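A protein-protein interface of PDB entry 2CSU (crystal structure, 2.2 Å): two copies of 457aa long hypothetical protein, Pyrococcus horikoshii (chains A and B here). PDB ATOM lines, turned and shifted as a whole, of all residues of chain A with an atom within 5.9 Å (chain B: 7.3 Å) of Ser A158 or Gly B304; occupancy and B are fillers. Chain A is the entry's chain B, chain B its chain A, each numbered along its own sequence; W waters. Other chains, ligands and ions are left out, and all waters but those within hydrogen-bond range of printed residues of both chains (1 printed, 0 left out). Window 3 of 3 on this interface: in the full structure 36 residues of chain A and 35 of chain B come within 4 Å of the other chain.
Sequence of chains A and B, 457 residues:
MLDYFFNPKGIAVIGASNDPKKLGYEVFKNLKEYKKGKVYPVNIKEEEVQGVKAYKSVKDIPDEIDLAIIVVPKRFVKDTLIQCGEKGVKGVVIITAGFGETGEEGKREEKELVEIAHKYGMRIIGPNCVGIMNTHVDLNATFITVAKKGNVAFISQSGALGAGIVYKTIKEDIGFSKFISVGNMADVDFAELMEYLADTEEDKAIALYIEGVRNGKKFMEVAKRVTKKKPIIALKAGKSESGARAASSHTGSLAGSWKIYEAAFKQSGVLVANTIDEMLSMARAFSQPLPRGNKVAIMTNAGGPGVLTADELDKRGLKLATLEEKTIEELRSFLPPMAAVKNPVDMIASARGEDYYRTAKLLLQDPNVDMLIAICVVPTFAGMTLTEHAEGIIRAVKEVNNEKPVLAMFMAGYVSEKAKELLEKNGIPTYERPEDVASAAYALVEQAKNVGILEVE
Among the printed residues, 8 pairs touch across the chains. Among the printed residues, no Asp or Glu carboxylate lies within 4 Å of a Lys or Arg side-chain nitrogen of the other chain.
Water W1 lies within hydrogen-bond range of the side-chain hydroxyl (OG) of Ser A158 (2.8 Å), the backbone NH (N) of Gly B304 (3.0 Å) and the backbone NH (N) of Gly B303 (3.3 Å).
No position is printed for both chains. Of the 8 pairs that touch across the chains among the printed residues, none has its exchanged pair printed and touching as well.
Of the printed residues of chain B, Leu A161 touches Pro B305 and Leu B308. Of the printed residues of chain B, Tyr A209 touches Gly B304 (3.7 Å) and Val B307 (3.4 Å). Of chain A, only Ser A158 and Tyr A209 come within 4 Å of Gly B304. Of the printed residues of chain A, Val B307 touches Tyr A209 (3.4 Å) and Ala A237 (3.3 Å). The nearest residue of chain B that does not touch Ser A158 is Pro B305 (4.5 Å). The nearest printed residue of chain A that does not touch Val B307 is Glu A211 (5.7 Å).
Among the printed residues, pairs that only touch across the chains: Ala A160 with Ala B302 (3.2 Å), Ala A237 with Val B307 (3.3 Å), Tyr A209 with Val B307 (3.4 Å), Tyr A209 with Gly B304 (3.7 Å), Leu A161 with Pro B305 (3.8 Å), Ser A158 with Gly B304 (3.8 Å), Leu A161 with Leu B308 (3.8 Å) and Ala A237 with Leu B308 (3.9 Å).
The backbone carbonyl oxygen (O) of Ala B302 sits at hydrogen-bond distance from the side-chain hydroxyl (OG1) of Thr B300. The backbone carbonyl oxygen (O) of Pro B305 is in hydrogen-bond range of the side-chain hydroxyl (OG1) of Thr B309, at 2.7 Å. The side-chain hydroxyl (OG) of Ser A156 is in hydrogen-bond range of the backbone carbonyl oxygen (O) of Ser A158, at 3.0 Å. The backbone carbonyl oxygen (O) of Tyr A209 is in hydrogen-bond range of the backbone NH (N) of Gln A157 (3.1 Å). OG of Ser A158 sits close to N of Leu A161 (3.2 Å).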
ATOM      1  N   SER A 156     -13.564  17.315 -28.008  1.00  0.00           N
ATOM      2  CA  SER A 156     -14.900  17.885 -27.903  1.00  0.00           C
ATOM      3  C   SER A 156     -15.586  17.981 -29.267  1.00  0.00           C
ATOM      4  O   SER A 156     -14.959  18.129 -30.308  1.00  0.00           O
ATOM      5  CB  SER A 156     -14.778  19.275 -27.280  1.00  0.00           C
ATOM      6  OG  SER A 156     -14.708  20.252 -28.317  1.00  0.00           O
ATOM      7  N   GLN A 157     -16.926  17.846 -29.237  1.00  0.00           N
ATOM      8  CA  GLN A 157     -17.691  17.931 -30.474  1.00  0.00           C
ATOM      9  C   GLN A 157     -17.982  19.384 -30.851  1.00  0.00           C
ATOM     10  O   GLN A 157     -18.477  19.698 -31.925  1.00  0.00           O
ATOM     11  CB  GLN A 157     -19.008  17.179 -30.269  1.00  0.00           C
ATOM     12  CG  GLN A 157     -18.969  15.764 -30.843  1.00  0.00           C
ATOM     13  CD  GLN A 157     -20.222  15.022 -30.439  1.00  0.00           C
ATOM     14  OE1 GLN A 157     -20.431  14.644 -29.298  1.00  0.00           O
ATOM     15  NE2 GLN A 157     -21.075  14.803 -31.459  1.00  0.00           N
ATOM     16  N   SER A 158     -17.694  20.286 -29.894  1.00  0.00           N
ATOM     17  CA  SER A 158     -17.943  21.701 -30.138  1.00  0.00           C
ATOM     18  C   SER A 158     -16.650  22.451 -30.471  1.00  0.00           C
ATOM     19  O   SER A 158     -15.808  22.711 -29.621  1.00  0.00           O
ATOM     20  CB  SER A 158     -18.581  22.294 -28.882  1.00  0.00           C
ATOM     21  OG  SER A 158     -18.688  23.710 -29.030  1.00  0.00           O
ATOM     22  N   GLY A 159     -16.493  22.764 -31.771  1.00  0.00           N
ATOM     23  CA  GLY A 159     -15.288  23.461 -32.208  1.00  0.00           C
ATOM     24  C   GLY A 159     -15.175  24.849 -31.576  1.00  0.00           C
ATOM     25  O   GLY A 159     -14.124  25.260 -31.104  1.00  0.00           O
ATOM     26  N   ALA A 160     -16.268  25.604 -31.552  1.00  0.00           N
ATOM     27  CA  ALA A 160     -16.263  26.944 -30.981  1.00  0.00           C
ATOM     28  C   ALA A 160     -15.835  26.899 -29.521  1.00  0.00           C
ATOM     29  O   ALA A 160     -14.957  27.652 -29.096  1.00  0.00           O
ATOM     30  CB  ALA A 160     -17.646  27.565 -31.098  1.00  0.00           C
ATOM     31  N   LEU A 161     -16.466  26.019 -28.755  1.00  0.00           N
ATOM     32  CA  LEU A 161     -16.131  25.872 -27.351  1.00  0.00           C
ATOM     33  C   LEU A 161     -14.712  25.313 -27.255  1.00  0.00           C
ATOM     34  O   LEU A 161     -13.981  25.609 -26.311  1.00  0.00           O
ATOM     35  CB  LEU A 161     -17.122  24.929 -26.669  1.00  0.00           C
ATOM     36  CG  LEU A 161     -16.996  24.789 -25.156  1.00  0.00           C
ATOM     37  CD1 LEU A 161     -17.131  26.151 -24.508  1.00  0.00           C
ATOM     38  CD2 LEU A 161     -18.074  23.856 -24.644  1.00  0.00           C
ATOM     39  N   GLY A 162     -14.330  24.512 -28.247  1.00  0.00           N
ATOM     40  CA  GLY A 162     -12.996  23.936 -28.264  1.00  0.00           C
ATOM     41  C   GLY A 162     -11.903  24.999 -28.301  1.00  0.00           C
ATOM     42  O   GLY A 162     -10.861  24.847 -27.670  1.00  0.00           O
ATOM     43  N   ALA A 163     -12.135  26.081 -29.038  1.00  0.00           N
ATOM     44  CA  ALA A 163     -11.150  27.157 -29.125  1.00  0.00           C
ATOM     45  C   ALA A 163     -11.229  28.030 -27.871  1.00  0.00           C
ATOM     46  O   ALA A 163     -10.208  28.474 -27.343  1.00  0.00           O
ATOM     47  CB  ALA A 163     -11.401  28.001 -30.371  1.00  0.00           C
ATOM     48  N   SER A 181     -10.541  18.316 -32.371  1.00  0.00           N
ATOM     49  CA  SER A 181     -11.842  18.866 -32.733  1.00  0.00           C
ATOM     50  C   SER A 181     -12.407  17.863 -33.734  1.00  0.00           C
ATOM     51  O   SER A 181     -11.936  17.807 -34.872  1.00  0.00           O
ATOM     52  CB  SER A 181     -11.682  20.229 -33.408  1.00  0.00           C
ATOM     53  OG  SER A 181     -12.947  20.763 -33.748  1.00  0.00           O
ATOM     54  N   TYR A 209     -15.799  16.803 -24.088  1.00  0.00           N
ATOM     55  CA  TYR A 209     -16.989  17.640 -24.120  1.00  0.00           C
ATOM     56  C   TYR A 209     -17.873  16.914 -25.116  1.00  0.00           C
ATOM     57  O   TYR A 209     -17.581  16.896 -26.309  1.00  0.00           O
ATOM     58  CB  TYR A 209     -16.717  19.042 -24.644  1.00  0.00           C
ATOM     59  CG  TYR A 209     -18.004  19.820 -24.802  1.00  0.00           C
ATOM     60  CD1 TYR A 209     -18.702  20.265 -23.687  1.00  0.00           C
ATOM     61  CD2 TYR A 209     -18.550  20.061 -26.060  1.00  0.00           C
ATOM     62  CE1 TYR A 209     -19.916  20.933 -23.811  1.00  0.00           C
ATOM     63  CE2 TYR A 209     -19.768  20.727 -26.200  1.00  0.00           C
ATOM     64  CZ  TYR A 209     -20.445  21.163 -25.068  1.00  0.00           C
ATOM     65  OH  TYR A 209     -21.637  21.847 -25.181  1.00  0.00           O
ATOM     66  N   GLU A 211     -21.716  16.139 -26.877  1.00  0.00           N
ATOM     67  CA  GLU A 211     -23.050  16.653 -27.171  1.00  0.00           C
ATOM     68  C   GLU A 211     -23.939  15.448 -27.472  1.00  0.00           C
ATOM     69  O   GLU A 211     -25.146  15.473 -27.232  1.00  0.00           O
ATOM     70  CB  GLU A 211     -23.023  17.577 -28.387  1.00  0.00           C
ATOM     71  CG  GLU A 211     -22.037  18.723 -28.283  1.00  0.00           C
ATOM     72  CD  GLU A 211     -22.084  19.636 -29.494  1.00  0.00           C
ATOM     73  OE1 GLU A 211     -22.044  19.113 -30.631  1.00  0.00           O
ATOM     74  OE2 GLU A 211     -22.156  20.872 -29.308  1.00  0.00           O
ATOM     75  N   ALA A 237     -23.340  18.387 -22.199  1.00  0.00           N
ATOM     76  CA  ALA A 237     -24.215  19.542 -22.346  1.00  0.00           C
ATOM     77  C   ALA A 237     -25.613  19.081 -22.738  1.00  0.00           C
ATOM     78  O   ALA A 237     -25.786  17.960 -23.216  1.00  0.00           O
ATOM     79  CB  ALA A 237     -23.663  20.473 -23.404  1.00  0.00           C
ATOM     80  N   THR B 300     -25.808  34.081 -29.463  1.00  0.00           N
ATOM     81  CA  THR B 300     -24.445  33.562 -29.422  1.00  0.00           C
ATOM     82  C   THR B 300     -23.870  33.286 -30.811  1.00  0.00           C
ATOM     83  O   THR B 300     -24.619  33.184 -31.793  1.00  0.00           O
ATOM     84  CB  THR B 300     -24.402  32.230 -28.622  1.00  0.00           C
ATOM     85  OG1 THR B 300     -23.060  31.764 -28.524  1.00  0.00           O
ATOM     86  CG2 THR B 300     -25.231  31.144 -29.337  1.00  0.00           C
ATOM     87  N   ASN B 301     -22.542  33.161 -30.881  1.00  0.00           N
ATOM     88  CA  ASN B 301     -21.861  32.852 -32.137  1.00  0.00           C
ATOM     89  C   ASN B 301     -21.302  31.437 -32.057  1.00  0.00           C
ATOM     90  O   ASN B 301     -20.608  30.973 -32.950  1.00  0.00           O
ATOM     91  CB  ASN B 301     -20.739  33.875 -32.412  1.00  0.00           C
ATOM     92  CG  ASN B 301     -19.534  33.716 -31.492  1.00  0.00           C
ATOM     93  OD1 ASN B 301     -19.641  33.238 -30.357  1.00  0.00           O
ATOM     94  ND2 ASN B 301     -18.372  34.149 -31.977  1.00  0.00           N
ATOM     95  N   ALA B 302     -21.635  30.751 -30.971  1.00  0.00           N
ATOM     96  CA  ALA B 302     -21.180  29.390 -30.725  1.00  0.00           C
ATOM     97  C   ALA B 302     -22.264  28.583 -30.013  1.00  0.00           C
ATOM     98  O   ALA B 302     -22.710  28.955 -28.925  1.00  0.00           O
ATOM     99  CB  ALA B 302     -19.918  29.415 -29.871  1.00  0.00           C
ATOM    100  N   GLY B 303     -22.685  27.483 -30.630  1.00  0.00           N
ATOM    101  CA  GLY B 303     -23.714  26.644 -30.033  1.00  0.00           C
ATOM    102  C   GLY B 303     -23.362  26.121 -28.645  1.00  0.00           C
ATOM    103  O   GLY B 303     -24.111  26.331 -27.696  1.00  0.00           O
ATOM    104  N   GLY B 304     -22.224  25.442 -28.532  1.00  0.00           N
ATOM    105  CA  GLY B 304     -21.797  24.884 -27.258  1.00  0.00           C
ATOM    106  C   GLY B 304     -22.021  25.807 -26.076  1.00  0.00           C
ATOM    107  O   GLY B 304     -22.815  25.496 -25.187  1.00  0.00           O
ATOM    108  N   PRO B 305     -21.325  26.954 -26.038  1.00  0.00           N
ATOM    109  CA  PRO B 305     -21.448  27.932 -24.962  1.00  0.00           C
ATOM    110  C   PRO B 305     -22.898  28.295 -24.680  1.00  0.00           C
ATOM    111  O   PRO B 305     -23.248  28.634 -23.564  1.00  0.00           O
ATOM    112  CB  PRO B 305     -20.650  29.121 -25.494  1.00  0.00           C
ATOM    113  CG  PRO B 305     -19.553  28.458 -26.234  1.00  0.00           C
ATOM    114  CD  PRO B 305     -20.272  27.357 -26.990  1.00  0.00           C
ATOM    115  N   GLY B 306     -23.733  28.247 -25.711  1.00  0.00           N
ATOM    116  CA  GLY B 306     -25.130  28.576 -25.537  1.00  0.00           C
ATOM    117  C   GLY B 306     -25.903  27.496 -24.791  1.00  0.00           C
ATOM    118  O   GLY B 306     -26.717  27.799 -23.912  1.00  0.00           O
ATOM    119  N   VAL B 307     -25.664  26.235 -25.141  1.00  0.00           N
ATOM    120  CA  VAL B 307     -26.371  25.135 -24.483  1.00  0.00           C
ATOM    121  C   VAL B 307     -25.961  25.081 -23.017  1.00  0.00           C
ATOM    122  O   VAL B 307     -26.803  24.959 -22.134  1.00  0.00           O
ATOM    123  CB  VAL B 307     -26.077  23.781 -25.168  1.00  0.00           C
ATOM    124  CG1 VAL B 307     -26.269  23.919 -26.665  1.00  0.00           C
ATOM    125  CG2 VAL B 307     -24.684  23.305 -24.840  1.00  0.00           C
ATOM    126  N   LEU B 308     -24.664  25.202 -22.755  1.00  0.00           N
ATOM    127  CA  LEU B 308     -24.190  25.199 -21.379  1.00  0.00           C
ATOM    128  C   LEU B 308     -24.851  26.355 -20.641  1.00  0.00           C
ATOM    129  O   LEU B 308     -25.364  26.178 -19.536  1.00  0.00           O
ATOM    130  CB  LEU B 308     -22.673  25.350 -21.326  1.00  0.00           C
ATOM    131  CG  LEU B 308     -21.852  24.126 -21.724  1.00  0.00           C
ATOM    132  CD1 LEU B 308     -20.369  24.468 -21.685  1.00  0.00           C
ATOM    133  CD2 LEU B 308     -22.162  22.967 -20.778  1.00  0.00           C
ATOM    134  N   THR B 309     -24.859  27.543 -21.244  1.00  0.00           N
ATOM    135  CA  THR B 309     -25.488  28.670 -20.566  1.00  0.00           C
ATOM    136  C   THR B 309     -26.977  28.427 -20.350  1.00  0.00           C
ATOM    137  O   THR B 309     -27.535  28.812 -19.319  1.00  0.00           O
ATOM    138  CB  THR B 309     -25.342  29.988 -21.337  1.00  0.00           C
ATOM    139  OG1 THR B 309     -23.953  30.298 -21.537  1.00  0.00           O
ATOM    140  CG2 THR B 309     -25.995  31.098 -20.548  1.00  0.00           C
ATOM    141  N   ALA B 310     -27.637  27.810 -21.320  1.00  0.00           N
ATOM    142  CA  ALA B 310     -29.068  27.537 -21.154  1.00  0.00           C
ATOM    143  C   ALA B 310     -29.254  26.595 -19.959  1.00  0.00           C
ATOM    144  O   ALA B 310     -30.076  26.846 -19.103  1.00  0.00           O
ATOM    145  CB  ALA B 310     -29.650  26.922 -22.424  1.00  0.00           C
ATOM    146  N   ASP B 346     -28.719  31.443 -32.431  1.00  0.00           N
ATOM    147  CA  ASP B 346     -27.335  31.088 -32.689  1.00  0.00           C
ATOM    148  C   ASP B 346     -26.841  31.598 -34.039  1.00  0.00           C
ATOM    149  O   ASP B 346     -26.868  30.900 -35.045  1.00  0.00           O
ATOM    150  CB  ASP B 346     -27.180  29.568 -32.611  1.00  0.00           C
ATOM    151  CG  ASP B 346     -25.708  29.224 -32.788  1.00  0.00           C
ATOM    152  OD1 ASP B 346     -25.396  28.032 -32.836  1.00  0.00           O
ATOM    153  OD2 ASP B 346     -24.902  30.141 -32.914  1.00  0.00           O
ATOM    154  N   ILE B 375     -23.466  35.996 -25.823  1.00  0.00           N
ATOM    155  CA  ILE B 375     -22.333  35.067 -25.734  1.00  0.00           C
ATOM    156  C   ILE B 375     -21.457  35.119 -26.998  1.00  0.00           C
ATOM    157  O   ILE B 375     -21.929  35.004 -28.127  1.00  0.00           O
ATOM    158  CB  ILE B 375     -22.896  33.652 -25.557  1.00  0.00           C
ATOM    159  CG1 ILE B 375     -23.713  33.564 -24.264  1.00  0.00           C
ATOM    160  CG2 ILE B 375     -21.744  32.632 -25.463  1.00  0.00           C
ATOM    161  CD1 ILE B 375     -24.395  32.203 -24.099  1.00  0.00           C
ATOM    162  N   PRO B 434     -20.262  29.988 -18.193  1.00  0.00           N
ATOM    163  CA  PRO B 434     -21.712  29.871 -18.344  1.00  0.00           C
ATOM    164  C   PRO B 434     -22.390  29.964 -16.976  1.00  0.00           C
ATOM    165  O   PRO B 434     -23.424  30.610 -16.837  1.00  0.00           O
ATOM    166  CB  PRO B 434     -21.875  28.497 -18.984  1.00  0.00           C
ATOM    167  CG  PRO B 434     -20.678  28.419 -19.866  1.00  0.00           C
ATOM    168  CD  PRO B 434     -19.574  28.931 -18.955  1.00  0.00           C
HETATM  169  O   HOH W   1     -20.277  25.213 -30.741  1.00  0.00           O
